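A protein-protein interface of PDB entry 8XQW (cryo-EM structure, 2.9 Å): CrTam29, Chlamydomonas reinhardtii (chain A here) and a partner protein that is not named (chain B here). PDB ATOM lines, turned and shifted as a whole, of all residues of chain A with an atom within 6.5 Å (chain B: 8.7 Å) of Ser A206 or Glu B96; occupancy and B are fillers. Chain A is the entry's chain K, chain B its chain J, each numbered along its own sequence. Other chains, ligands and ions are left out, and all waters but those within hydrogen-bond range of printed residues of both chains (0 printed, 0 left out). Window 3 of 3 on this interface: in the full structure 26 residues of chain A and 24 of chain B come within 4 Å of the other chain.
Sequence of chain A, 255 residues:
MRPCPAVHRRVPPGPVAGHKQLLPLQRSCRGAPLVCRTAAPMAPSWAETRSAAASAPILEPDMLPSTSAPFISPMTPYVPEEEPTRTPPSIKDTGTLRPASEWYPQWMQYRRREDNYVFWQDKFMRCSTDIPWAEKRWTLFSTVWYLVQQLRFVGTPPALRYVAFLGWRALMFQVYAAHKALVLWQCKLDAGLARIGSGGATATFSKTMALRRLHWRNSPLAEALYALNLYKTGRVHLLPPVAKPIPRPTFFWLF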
ATOM      1  N   CYS A 187       8.184  38.899  23.564  1.00  0.00           N
ATOM      2  CA  CYS A 187       9.465  38.256  23.841  1.00  0.00           C
ATOM      3  C   CYS A 187      10.586  39.282  23.874  1.00  0.00           C
ATOM      4  O   CYS A 187      11.414  39.291  24.796  1.00  0.00           O
ATOM      5  CB  CYS A 187       9.753  37.188  22.795  1.00  0.00           C
ATOM      6  SG  CYS A 187       8.869  35.653  23.060  1.00  0.00           S
ATOM      7  N   ASP A 190      10.210  41.502  27.209  1.00  0.00           N
ATOM      8  CA  ASP A 190      10.620  40.909  28.472  1.00  0.00           C
ATOM      9  C   ASP A 190      12.106  40.585  28.485  1.00  0.00           C
ATOM     10  O   ASP A 190      12.742  40.654  29.545  1.00  0.00           O
ATOM     11  CB  ASP A 190       9.781  39.672  28.776  1.00  0.00           C
ATOM     12  CG  ASP A 190      10.185  38.466  27.964  1.00  0.00           C
ATOM     13  OD1 ASP A 190      11.275  37.906  28.203  1.00  0.00           O
ATOM     14  OD2 ASP A 190       9.393  38.062  27.091  1.00  0.00           O
ATOM     15  N   THR A 204      18.660  37.328  27.492  1.00  0.00           N
ATOM     16  CA  THR A 204      17.859  36.296  26.860  1.00  0.00           C
ATOM     17  C   THR A 204      16.393  36.431  27.249  1.00  0.00           C
ATOM     18  O   THR A 204      15.993  37.354  27.959  1.00  0.00           O
ATOM     19  CB  THR A 204      18.359  34.911  27.254  1.00  0.00           C
ATOM     20  OG1 THR A 204      18.790  34.935  28.618  1.00  0.00           O
ATOM     21  CG2 THR A 204      19.515  34.493  26.371  1.00  0.00           C
ATOM     22  N   PHE A 205      15.593  35.502  26.759  1.00  0.00           N
ATOM     23  CA  PHE A 205      14.230  35.315  27.219  1.00  0.00           C
ATOM     24  C   PHE A 205      13.996  33.819  27.404  1.00  0.00           C
ATOM     25  O   PHE A 205      14.918  33.010  27.292  1.00  0.00           O
ATOM     26  CB  PHE A 205      13.232  35.946  26.250  1.00  0.00           C
ATOM     27  CG  PHE A 205      13.320  35.412  24.860  1.00  0.00           C
ATOM     28  CD1 PHE A 205      12.666  34.251  24.506  1.00  0.00           C
ATOM     29  CD2 PHE A 205      14.049  36.075  23.903  1.00  0.00           C
ATOM     30  CE1 PHE A 205      12.750  33.759  23.232  1.00  0.00           C
ATOM     31  CE2 PHE A 205      14.131  35.586  22.627  1.00  0.00           C
ATOM     32  CZ  PHE A 205      13.480  34.427  22.295  1.00  0.00           C
ATOM     33  N   SER A 206      12.755  33.451  27.685  1.00  0.00           N
ATOM     34  CA  SER A 206      12.388  32.061  27.889  1.00  0.00           C
ATOM     35  C   SER A 206      11.537  31.594  26.724  1.00  0.00           C
ATOM     36  O   SER A 206      10.481  32.170  26.458  1.00  0.00           O
ATOM     37  CB  SER A 206      11.628  31.889  29.198  1.00  0.00           C
ATOM     38  OG  SER A 206      11.905  30.628  29.775  1.00  0.00           O
ATOM     39  N   LYS A 207      11.999  30.559  26.022  1.00  0.00           N
ATOM     40  CA  LYS A 207      11.196  30.011  24.938  1.00  0.00           C
ATOM     41  C   LYS A 207       9.971  29.294  25.470  1.00  0.00           C
ATOM     42  O   LYS A 207       8.920  29.288  24.818  1.00  0.00           O
ATOM     43  CB  LYS A 207      12.029  29.064  24.089  1.00  0.00           C
ATOM     44  CG  LYS A 207      13.301  29.678  23.556  1.00  0.00           C
ATOM     45  CD  LYS A 207      14.177  28.622  22.929  1.00  0.00           C
ATOM     46  CE  LYS A 207      15.542  29.172  22.594  1.00  0.00           C
ATOM     47  NZ  LYS A 207      16.522  28.064  22.494  1.00  0.00           N
ATOM     48  N   THR A 208      10.095  28.675  26.644  1.00  0.00           N
ATOM     49  CA  THR A 208       8.946  28.067  27.291  1.00  0.00           C
ATOM     50  C   THR A 208       7.820  29.068  27.448  1.00  0.00           C
ATOM     51  O   THR A 208       6.662  28.766  27.150  1.00  0.00           O
ATOM     52  CB  THR A 208       9.351  27.517  28.648  1.00  0.00           C
ATOM     53  OG1 THR A 208      10.483  26.661  28.490  1.00  0.00           O
ATOM     54  CG2 THR A 208       8.225  26.736  29.253  1.00  0.00           C
ATOM     55  N   MET A 209       8.139  30.277  27.900  1.00  0.00           N
ATOM     56  CA  MET A 209       7.089  31.258  28.091  1.00  0.00           C
ATOM     57  C   MET A 209       6.516  31.727  26.768  1.00  0.00           C
ATOM     58  O   MET A 209       5.320  32.008  26.686  1.00  0.00           O
ATOM     59  CB  MET A 209       7.608  32.435  28.897  1.00  0.00           C
ATOM     60  CG  MET A 209       6.512  33.226  29.559  1.00  0.00           C
ATOM     61  SD  MET A 209       5.660  32.285  30.824  1.00  0.00           S
ATOM     62  CE  MET A 209       4.467  33.486  31.387  1.00  0.00           C
ATOM     63  N   ALA A 210       7.331  31.796  25.718  1.00  0.00           N
ATOM     64  CA  ALA A 210       6.800  32.164  24.411  1.00  0.00           C
ATOM     65  C   ALA A 210       5.774  31.146  23.938  1.00  0.00           C
ATOM     66  O   ALA A 210       4.662  31.507  23.527  1.00  0.00           O
ATOM     67  CB  ALA A 210       7.935  32.285  23.403  1.00  0.00           C
ATOM     68  N   LEU A 211       6.122  29.863  24.014  1.00  0.00           N
ATOM     69  CA  LEU A 211       5.188  28.828  23.592  1.00  0.00           C
ATOM     70  C   LEU A 211       3.958  28.776  24.484  1.00  0.00           C
ATOM     71  O   LEU A 211       2.864  28.481  24.003  1.00  0.00           O
ATOM     72  CB  LEU A 211       5.884  27.478  23.577  1.00  0.00           C
ATOM     73  CG  LEU A 211       7.095  27.473  22.657  1.00  0.00           C
ATOM     74  CD1 LEU A 211       7.914  26.238  22.885  1.00  0.00           C
ATOM     75  CD2 LEU A 211       6.650  27.552  21.220  1.00  0.00           C
ATOM     76  N   ARG A 213       2.620  31.362  25.923  1.00  0.00           N
ATOM     77  CA  ARG A 213       1.817  32.513  25.542  1.00  0.00           C
ATOM     78  C   ARG A 213       1.068  32.256  24.248  1.00  0.00           C
ATOM     79  O   ARG A 213      -0.037  32.766  24.053  1.00  0.00           O
ATOM     80  CB  ARG A 213       2.708  33.738  25.402  1.00  0.00           C
ATOM     81  CG  ARG A 213       2.811  34.553  26.649  1.00  0.00           C
ATOM     82  CD  ARG A 213       3.390  35.903  26.353  1.00  0.00           C
ATOM     83  NE  ARG A 213       4.842  35.872  26.395  1.00  0.00           N
ATOM     84  CZ  ARG A 213       5.553  36.176  27.470  1.00  0.00           C
ATOM     85  NH1 ARG A 213       4.942  36.535  28.584  1.00  0.00           N
ATOM     86  NH2 ARG A 213       6.875  36.123  27.426  1.00  0.00           N
ATOM     87  N   TYR A 226       5.056  37.283  36.631  1.00  0.00           N
ATOM     88  CA  TYR A 226       6.294  37.000  35.915  1.00  0.00           C
ATOM     89  C   TYR A 226       7.012  38.280  35.540  1.00  0.00           C
ATOM     90  O   TYR A 226       8.232  38.379  35.691  1.00  0.00           O
ATOM     91  CB  TYR A 226       6.013  36.185  34.664  1.00  0.00           C
ATOM     92  CG  TYR A 226       7.248  35.807  33.893  1.00  0.00           C
ATOM     93  CD1 TYR A 226       8.292  35.150  34.504  1.00  0.00           C
ATOM     94  CD2 TYR A 226       7.359  36.092  32.550  1.00  0.00           C
ATOM     95  CE1 TYR A 226       9.409  34.794  33.804  1.00  0.00           C
ATOM     96  CE2 TYR A 226       8.478  35.743  31.843  1.00  0.00           C
ATOM     97  CZ  TYR A 226       9.496  35.094  32.477  1.00  0.00           C
ATOM     98  OH  TYR A 226      10.617  34.741  31.778  1.00  0.00           O
ATOM     99  N   VAL A 236      15.204  34.692  34.575  1.00  0.00           N
ATOM    100  CA  VAL A 236      14.289  34.542  33.461  1.00  0.00           C
ATOM    101  C   VAL A 236      13.683  33.148  33.406  1.00  0.00           C
ATOM    102  O   VAL A 236      12.700  32.939  32.694  1.00  0.00           O
ATOM    103  CB  VAL A 236      15.023  34.896  32.155  1.00  0.00           C
ATOM    104  CG1 VAL A 236      15.709  33.689  31.590  1.00  0.00           C
ATOM    105  CG2 VAL A 236      14.079  35.494  31.154  1.00  0.00           C
ATOM    106  N   HIS A 237      14.217  32.190  34.156  1.00  0.00           N
ATOM    107  CA  HIS A 237      13.785  30.802  34.052  1.00  0.00           C
ATOM    108  C   HIS A 237      12.832  30.379  35.160  1.00  0.00           C
ATOM    109  O   HIS A 237      12.549  29.186  35.290  1.00  0.00           O
ATOM    110  CB  HIS A 237      14.994  29.875  34.036  1.00  0.00           C
ATOM    111  CG  HIS A 237      15.710  29.845  32.725  1.00  0.00           C
ATOM    112  ND1 HIS A 237      15.266  30.535  31.620  1.00  0.00           N
ATOM    113  CD2 HIS A 237      16.841  29.209  32.339  1.00  0.00           C
ATOM    114  CE1 HIS A 237      16.094  30.332  30.613  1.00  0.00           C
ATOM    115  NE2 HIS A 237      17.058  29.529  31.023  1.00  0.00           N
ATOM    116  N   LEU A 238      12.330  31.315  35.955  1.00  0.00           N
ATOM    117  CA  LEU A 238      11.355  31.014  36.998  1.00  0.00           C
ATOM    118  C   LEU A 238       9.964  31.313  36.459  1.00  0.00           C
ATOM    119  O   LEU A 238       9.601  32.477  36.277  1.00  0.00           O
ATOM    120  CB  LEU A 238      11.643  31.836  38.245  1.00  0.00           C
ATOM    121  CG  LEU A 238      12.203  31.078  39.434  1.00  0.00           C
ATOM    122  CD1 LEU A 238      12.049  31.919  40.666  1.00  0.00           C
ATOM    123  CD2 LEU A 238      11.482  29.772  39.597  1.00  0.00           C
ATOM    124  N   LEU A 239       9.175  30.271  36.228  1.00  0.00           N
ATOM    125  CA  LEU A 239       7.930  30.482  35.520  1.00  0.00           C
ATOM    126  C   LEU A 239       6.726  30.216  36.412  1.00  0.00           C
ATOM    127  O   LEU A 239       6.764  29.326  37.263  1.00  0.00           O
ATOM    128  CB  LEU A 239       7.862  29.574  34.290  1.00  0.00           C
ATOM    129  CG  LEU A 239       8.948  29.783  33.240  1.00  0.00           C
ATOM    130  CD1 LEU A 239       9.146  28.516  32.455  1.00  0.00           C
ATOM    131  CD2 LEU A 239       8.573  30.907  32.320  1.00  0.00           C
ATOM    132  O   4HH B  72      15.140  32.799  18.732  1.00  0.00           O
ATOM    133  C   4HH B  72      15.893  33.726  18.992  1.00  0.00           C
ATOM    134  CA  4HH B  72      17.213  33.389  19.668  1.00  0.00           C
ATOM    135  N   4HH B  72      18.389  33.697  18.816  1.00  0.00           N
ATOM    136  CB  4HH B  72      17.323  34.123  20.964  1.00  0.00           C
ATOM    137  OG  4HH B  72      17.890  35.430  20.718  1.00  0.00           O
ATOM    138  CJ  4HH B  72      17.353  38.101  20.550  1.00  0.00           C
ATOM    139  CK  4HH B  72      17.459  39.616  20.471  1.00  0.00           C
ATOM    140  CL1 4HH B  72      17.335  40.048  19.008  1.00  0.00           C
ATOM    141  CL2 4HH B  72      18.824  40.054  21.005  1.00  0.00           C
ATOM    142  CL3 4HH B  72      16.417  41.762  21.420  1.00  0.00           C
ATOM    143  CM  4HH B  72      16.347  40.246  21.313  1.00  0.00           C
ATOM    144  OM  4HH B  72      16.442  39.665  22.600  1.00  0.00           O
ATOM    145  NN  4HH B  72      16.819  42.271  22.575  1.00  0.00           N
ATOM    146  ON  4HH B  72      16.085  42.463  20.467  1.00  0.00           O
ATOM    147  P   4HH B  72      18.550  36.230  21.943  1.00  0.00           P
ATOM    148  O1P 4HH B  72      20.019  36.363  21.663  1.00  0.00           O
ATOM    149  O2P 4HH B  72      18.078  35.617  23.229  1.00  0.00           O
ATOM    150  O3P 4HH B  72      17.881  37.683  21.829  1.00  0.00           O
ATOM    151  CO  4HH B  72      16.726  43.691  22.890  1.00  0.00           C
ATOM    152  CP  4HH B  72      15.336  44.094  23.322  1.00  0.00           C
ATOM    153  CQ  4HH B  72      14.743  45.140  22.402  1.00  0.00           C
ATOM    154  CS  4HH B  72      13.499  46.062  24.308  1.00  0.00           C
ATOM    155  CT  4HH B  72      12.220  46.847  24.421  1.00  0.00           C
ATOM    156  NR  4HH B  72      14.068  46.141  22.972  1.00  0.00           N
ATOM    157  OR  4HH B  72      14.882  45.064  21.185  1.00  0.00           O
ATOM    158  SU  4HH B  72      11.781  47.653  22.859  1.00  0.00           S
ATOM    159  N   THR B  75      14.970  31.074  16.725  1.00  0.00           N
ATOM    160  CA  THR B  75      14.861  29.654  17.032  1.00  0.00           C
ATOM    161  C   THR B  75      13.479  29.521  17.588  1.00  0.00           C
ATOM    162  O   THR B  75      13.109  28.411  17.952  1.00  0.00           O
ATOM    163  CB  THR B  75      15.913  29.196  18.026  1.00  0.00           C
ATOM    164  OG1 THR B  75      17.076  29.924  17.656  1.00  0.00           O
ATOM    165  CG2 THR B  75      16.192  27.710  17.938  1.00  0.00           C
ATOM    166  N   VAL B  76      12.738  30.625  17.671  1.00  0.00           N
ATOM    167  CA  VAL B  76      11.327  30.576  18.142  1.00  0.00           C
ATOM    168  C   VAL B  76      10.447  30.556  16.901  1.00  0.00           C
ATOM    169  O   VAL B  76       9.663  29.642  16.778  1.00  0.00           O
ATOM    170  CB  VAL B  76      10.881  31.716  19.064  1.00  0.00           C
ATOM    171  CG1 VAL B  76      10.606  31.209  20.470  1.00  0.00           C
ATOM    172  CG2 VAL B  76      11.877  32.857  19.101  1.00  0.00           C
ATOM    173  N   MET B  79      10.245  27.324  15.567  1.00  0.00           N
ATOM    174  CA  MET B  79       9.331  26.452  16.302  1.00  0.00           C
ATOM    175  C   MET B  79       7.885  26.702  15.903  1.00  0.00           C
ATOM    176  O   MET B  79       7.099  25.760  15.744  1.00  0.00           O
ATOM    177  CB  MET B  79       9.494  26.648  17.804  1.00  0.00           C
ATOM    178  CG  MET B  79      10.849  26.275  18.333  1.00  0.00           C
ATOM    179  SD  MET B  79      11.339  24.621  17.854  1.00  0.00           S
ATOM    180  CE  MET B  79      12.939  24.947  17.130  1.00  0.00           C
ATOM    181  N   LEU B  90       3.778  21.640  20.811  1.00  0.00           N
ATOM    182  CA  LEU B  90       5.051  21.181  21.345  1.00  0.00           C
ATOM    183  C   LEU B  90       5.018  21.154  22.863  1.00  0.00           C
ATOM    184  O   LEU B  90       4.381  21.996  23.499  1.00  0.00           O
ATOM    185  CB  LEU B  90       6.189  22.086  20.877  1.00  0.00           C
ATOM    186  CG  LEU B  90       6.658  21.923  19.438  1.00  0.00           C
ATOM    187  CD1 LEU B  90       7.469  23.126  19.027  1.00  0.00           C
ATOM    188  CD2 LEU B  90       7.475  20.659  19.295  1.00  0.00           C
ATOM    189  N   GLU B  91       5.705  20.176  23.442  1.00  0.00           N
ATOM    190  CA  GLU B  91       5.874  20.147  24.883  1.00  0.00           C
ATOM    191  C   GLU B  91       6.935  21.168  25.268  1.00  0.00           C
ATOM    192  O   GLU B  91       8.081  21.080  24.822  1.00  0.00           O
ATOM    193  CB  GLU B  91       6.274  18.741  25.330  1.00  0.00           C
ATOM    194  CG  GLU B  91       6.188  18.485  26.821  1.00  0.00           C
ATOM    195  CD  GLU B  91       7.298  19.141  27.610  1.00  0.00           C
ATOM    196  OE1 GLU B  91       8.475  18.981  27.225  1.00  0.00           O
ATOM    197  OE2 GLU B  91       6.989  19.816  28.613  1.00  0.00           O
ATOM    198  N   GLU B  92       6.553  22.141  26.098  1.00  0.00           N
ATOM    199  CA  GLU B  92       7.382  23.330  26.274  1.00  0.00           C
ATOM    200  C   GLU B  92       8.659  23.045  27.050  1.00  0.00           C
ATOM    201  O   GLU B  92       9.736  23.541  26.680  1.00  0.00           O
ATOM    202  CB  GLU B  92       6.575  24.421  26.969  1.00  0.00           C
ATOM    203  CG  GLU B  92       5.291  24.774  26.262  1.00  0.00           C
ATOM    204  CD  GLU B  92       4.075  24.255  26.993  1.00  0.00           C
ATOM    205  OE1 GLU B  92       2.957  24.361  26.451  1.00  0.00           O
ATOM    206  OE2 GLU B  92       4.240  23.735  28.116  1.00  0.00           O
ATOM    207  N   GLU B  93       8.563  22.268  28.130  1.00  0.00           N
ATOM    208  CA  GLU B  93       9.731  22.014  28.969  1.00  0.00           C
ATOM    209  C   GLU B  93      10.881  21.448  28.148  1.00  0.00           C
ATOM    210  O   GLU B  93      12.021  21.913  28.251  1.00  0.00           O
ATOM    211  CB  GLU B  93       9.370  21.061  30.107  1.00  0.00           C
ATOM    212  CG  GLU B  93       8.342  21.598  31.089  1.00  0.00           C
ATOM    213  CD  GLU B  93       8.559  23.057  31.444  1.00  0.00           C
ATOM    214  OE1 GLU B  93       9.696  23.426  31.807  1.00  0.00           O
ATOM    215  OE2 GLU B  93       7.585  23.834  31.369  1.00  0.00           O
ATOM    216  N   GLY B  94      10.598  20.443  27.322  1.00  0.00           N
ATOM    217  CA  GLY B  94      11.612  19.933  26.421  1.00  0.00           C
ATOM    218  C   GLY B  94      11.951  20.890  25.304  1.00  0.00           C
ATOM    219  O   GLY B  94      13.075  20.866  24.795  1.00  0.00           O
ATOM    220  N   ALA B  95      11.008  21.743  24.918  1.00  0.00           N
ATOM    221  CA  ALA B  95      11.268  22.705  23.859  1.00  0.00           C
ATOM    222  C   ALA B  95      12.231  23.797  24.289  1.00  0.00           C
ATOM    223  O   ALA B  95      12.720  24.542  23.439  1.00  0.00           O
ATOM    224  CB  ALA B  95       9.960  23.334  23.384  1.00  0.00           C
ATOM    225  N   GLU B  96      12.505  23.920  25.583  1.00  0.00           N
ATOM    226  CA  GLU B  96      13.507  24.895  25.995  1.00  0.00           C
ATOM    227  C   GLU B  96      14.915  24.490  25.574  1.00  0.00           C
ATOM    228  O   GLU B  96      15.778  25.359  25.419  1.00  0.00           O
ATOM    229  CB  GLU B  96      13.447  25.100  27.508  1.00  0.00           C
ATOM    230  CG  GLU B  96      14.417  26.142  28.044  1.00  0.00           C
ATOM    231  CD  GLU B  96      13.796  27.520  28.152  1.00  0.00           C
ATOM    232  OE1 GLU B  96      13.055  27.764  29.129  1.00  0.00           O
ATOM    233  OE2 GLU B  96      14.052  28.362  27.267  1.00  0.00           O
ATOM    234  N   LYS B  97      15.164  23.203  25.354  1.00  0.00           N
ATOM    235  CA  LYS B  97      16.502  22.676  25.114  1.00  0.00           C
ATOM    236  C   LYS B  97      16.641  22.091  23.715  1.00  0.00           C
ATOM    237  O   LYS B  97      17.173  20.998  23.530  1.00  0.00           O
ATOM    238  CB  LYS B  97      16.864  21.625  26.156  1.00  0.00           C
ATOM    239  CG  LYS B  97      16.399  21.968  27.544  1.00  0.00           C
ATOM    240  CD  LYS B  97      16.004  20.726  28.311  1.00  0.00           C
ATOM    241  CE  LYS B  97      15.259  21.096  29.578  1.00  0.00           C
ATOM    242  NZ  LYS B  97      14.806  19.898  30.323  1.00  0.00           N
ATOM    243  N   ILE B  98      16.150  22.802  22.710  1.00  0.00           N
ATOM    244  CA  ILE B  98      16.275  22.385  21.320  1.00  0.00           C
ATOM    245  C   ILE B  98      17.416  23.173  20.694  1.00  0.00           C
ATOM    246  O   ILE B  98      17.349  24.402  20.587  1.00  0.00           O
ATOM    247  CB  ILE B  98      14.963  22.598  20.553  1.00  0.00           C
ATOM    248  CG1 ILE B  98      14.000  21.452  20.845  1.00  0.00           C
ATOM    249  CG2 ILE B  98      15.223  22.684  19.072  1.00  0.00           C
ATOM    250  CD1 ILE B  98      12.763  21.462  19.987  1.00  0.00           C
ATOM    251  N   ALA B  99      18.475  22.470  20.292  1.00  0.00           N
ATOM    252  CA  ALA B  99      19.640  23.119  19.717  1.00  0.00           C
ATOM    253  C   ALA B  99      20.164  22.465  18.452  1.00  0.00           C
ATOM    254  O   ALA B  99      20.957  23.096  17.749  1.00  0.00           O
ATOM    255  CB  ALA B  99      20.781  23.179  20.741  1.00  0.00           C
ATOM    256  N   MET B 107      11.500  15.548  18.929  1.00  0.00           N
ATOM    257  CA  MET B 107      10.391  16.162  19.643  1.00  0.00           C
ATOM    258  C   MET B 107       9.104  16.026  18.850  1.00  0.00           C
ATOM    259  O   MET B 107       8.076  15.583  19.373  1.00  0.00           O
ATOM    260  CB  MET B 107      10.702  17.634  19.905  1.00  0.00           C
ATOM    261  CG  MET B 107      10.194  18.149  21.224  1.00  0.00           C
ATOM    262  SD  MET B 107      10.960  17.281  22.601  1.00  0.00           S
ATOM    263  CE  MET B 107      12.691  17.443  22.179  1.00  0.00           C
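OE1 of Glu B96 sits at hydrogen-bond distance from OG1 of Thr A208 (2.9 Å). OG of Ser A206 is in hydrogen-bond range of OE1 of Glu B96, at 3.2 Å. The backbone NH (N) of Lys A207 lies within hydrogen-bond range of the side-chain carboxylate (OE2) of Glu B96, 3.3 Å away.
N of Glu B93 is in hydrogen-bond range of OE2 of Glu B91, 3.0 Å away.
CG2 of Thr A204 touches O2P of 4HH B72 (3.6 Å). Phe A205 touches 4HH B72 (CE2 to CB, 3.9 Å). Phe A205 touches Val B76. Thr A208 touches Glu B92 (CG2 to CB, 3.6 Å). CG2 of Thr A208 touches OE2 of Glu B93 (3.6 Å). Leu A211 touches Glu B92. Leu A211 touches Ala B95 (CD1 to CB, 3.6 Å).
Printed residues of chain B within 4 Å of Phe A205: 4HH B72 (3.9 Å) and Val B76 (3.9 Å). Printed residues of chain B within 4 Å of Ser A206: Glu B96 (3.2 Å). Printed residues of chain B within 4 Å of Lys A207: Glu B96 (3.3 Å). Printed residues of chain A within 4 Å of 4HH B72: Thr A204 and Phe A205. Printed residues of chain A within 4 Å of Glu B92: Thr A208 (3.6 Å) and Leu A211 (3.9 Å). Of the printed residues of chain A, Glu B93 touches Thr A208. Of chain A, only Ser A206 (3.2 Å), Lys A207 (3.3 Å) and Thr A208 (2.9 Å) come within 4 Å of Glu B96. The nearest printed residue of chain A that does not touch Glu B92 is Lys A207 (5.8 Å).
Hydrophobic or aromatic side chains of chain A that line the printed part of chain B: Phe A205 and Leu A211. Hydrophobic or aromatic side chains of chain B that line the printed part of chain A: Val B76 and Ala B95.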
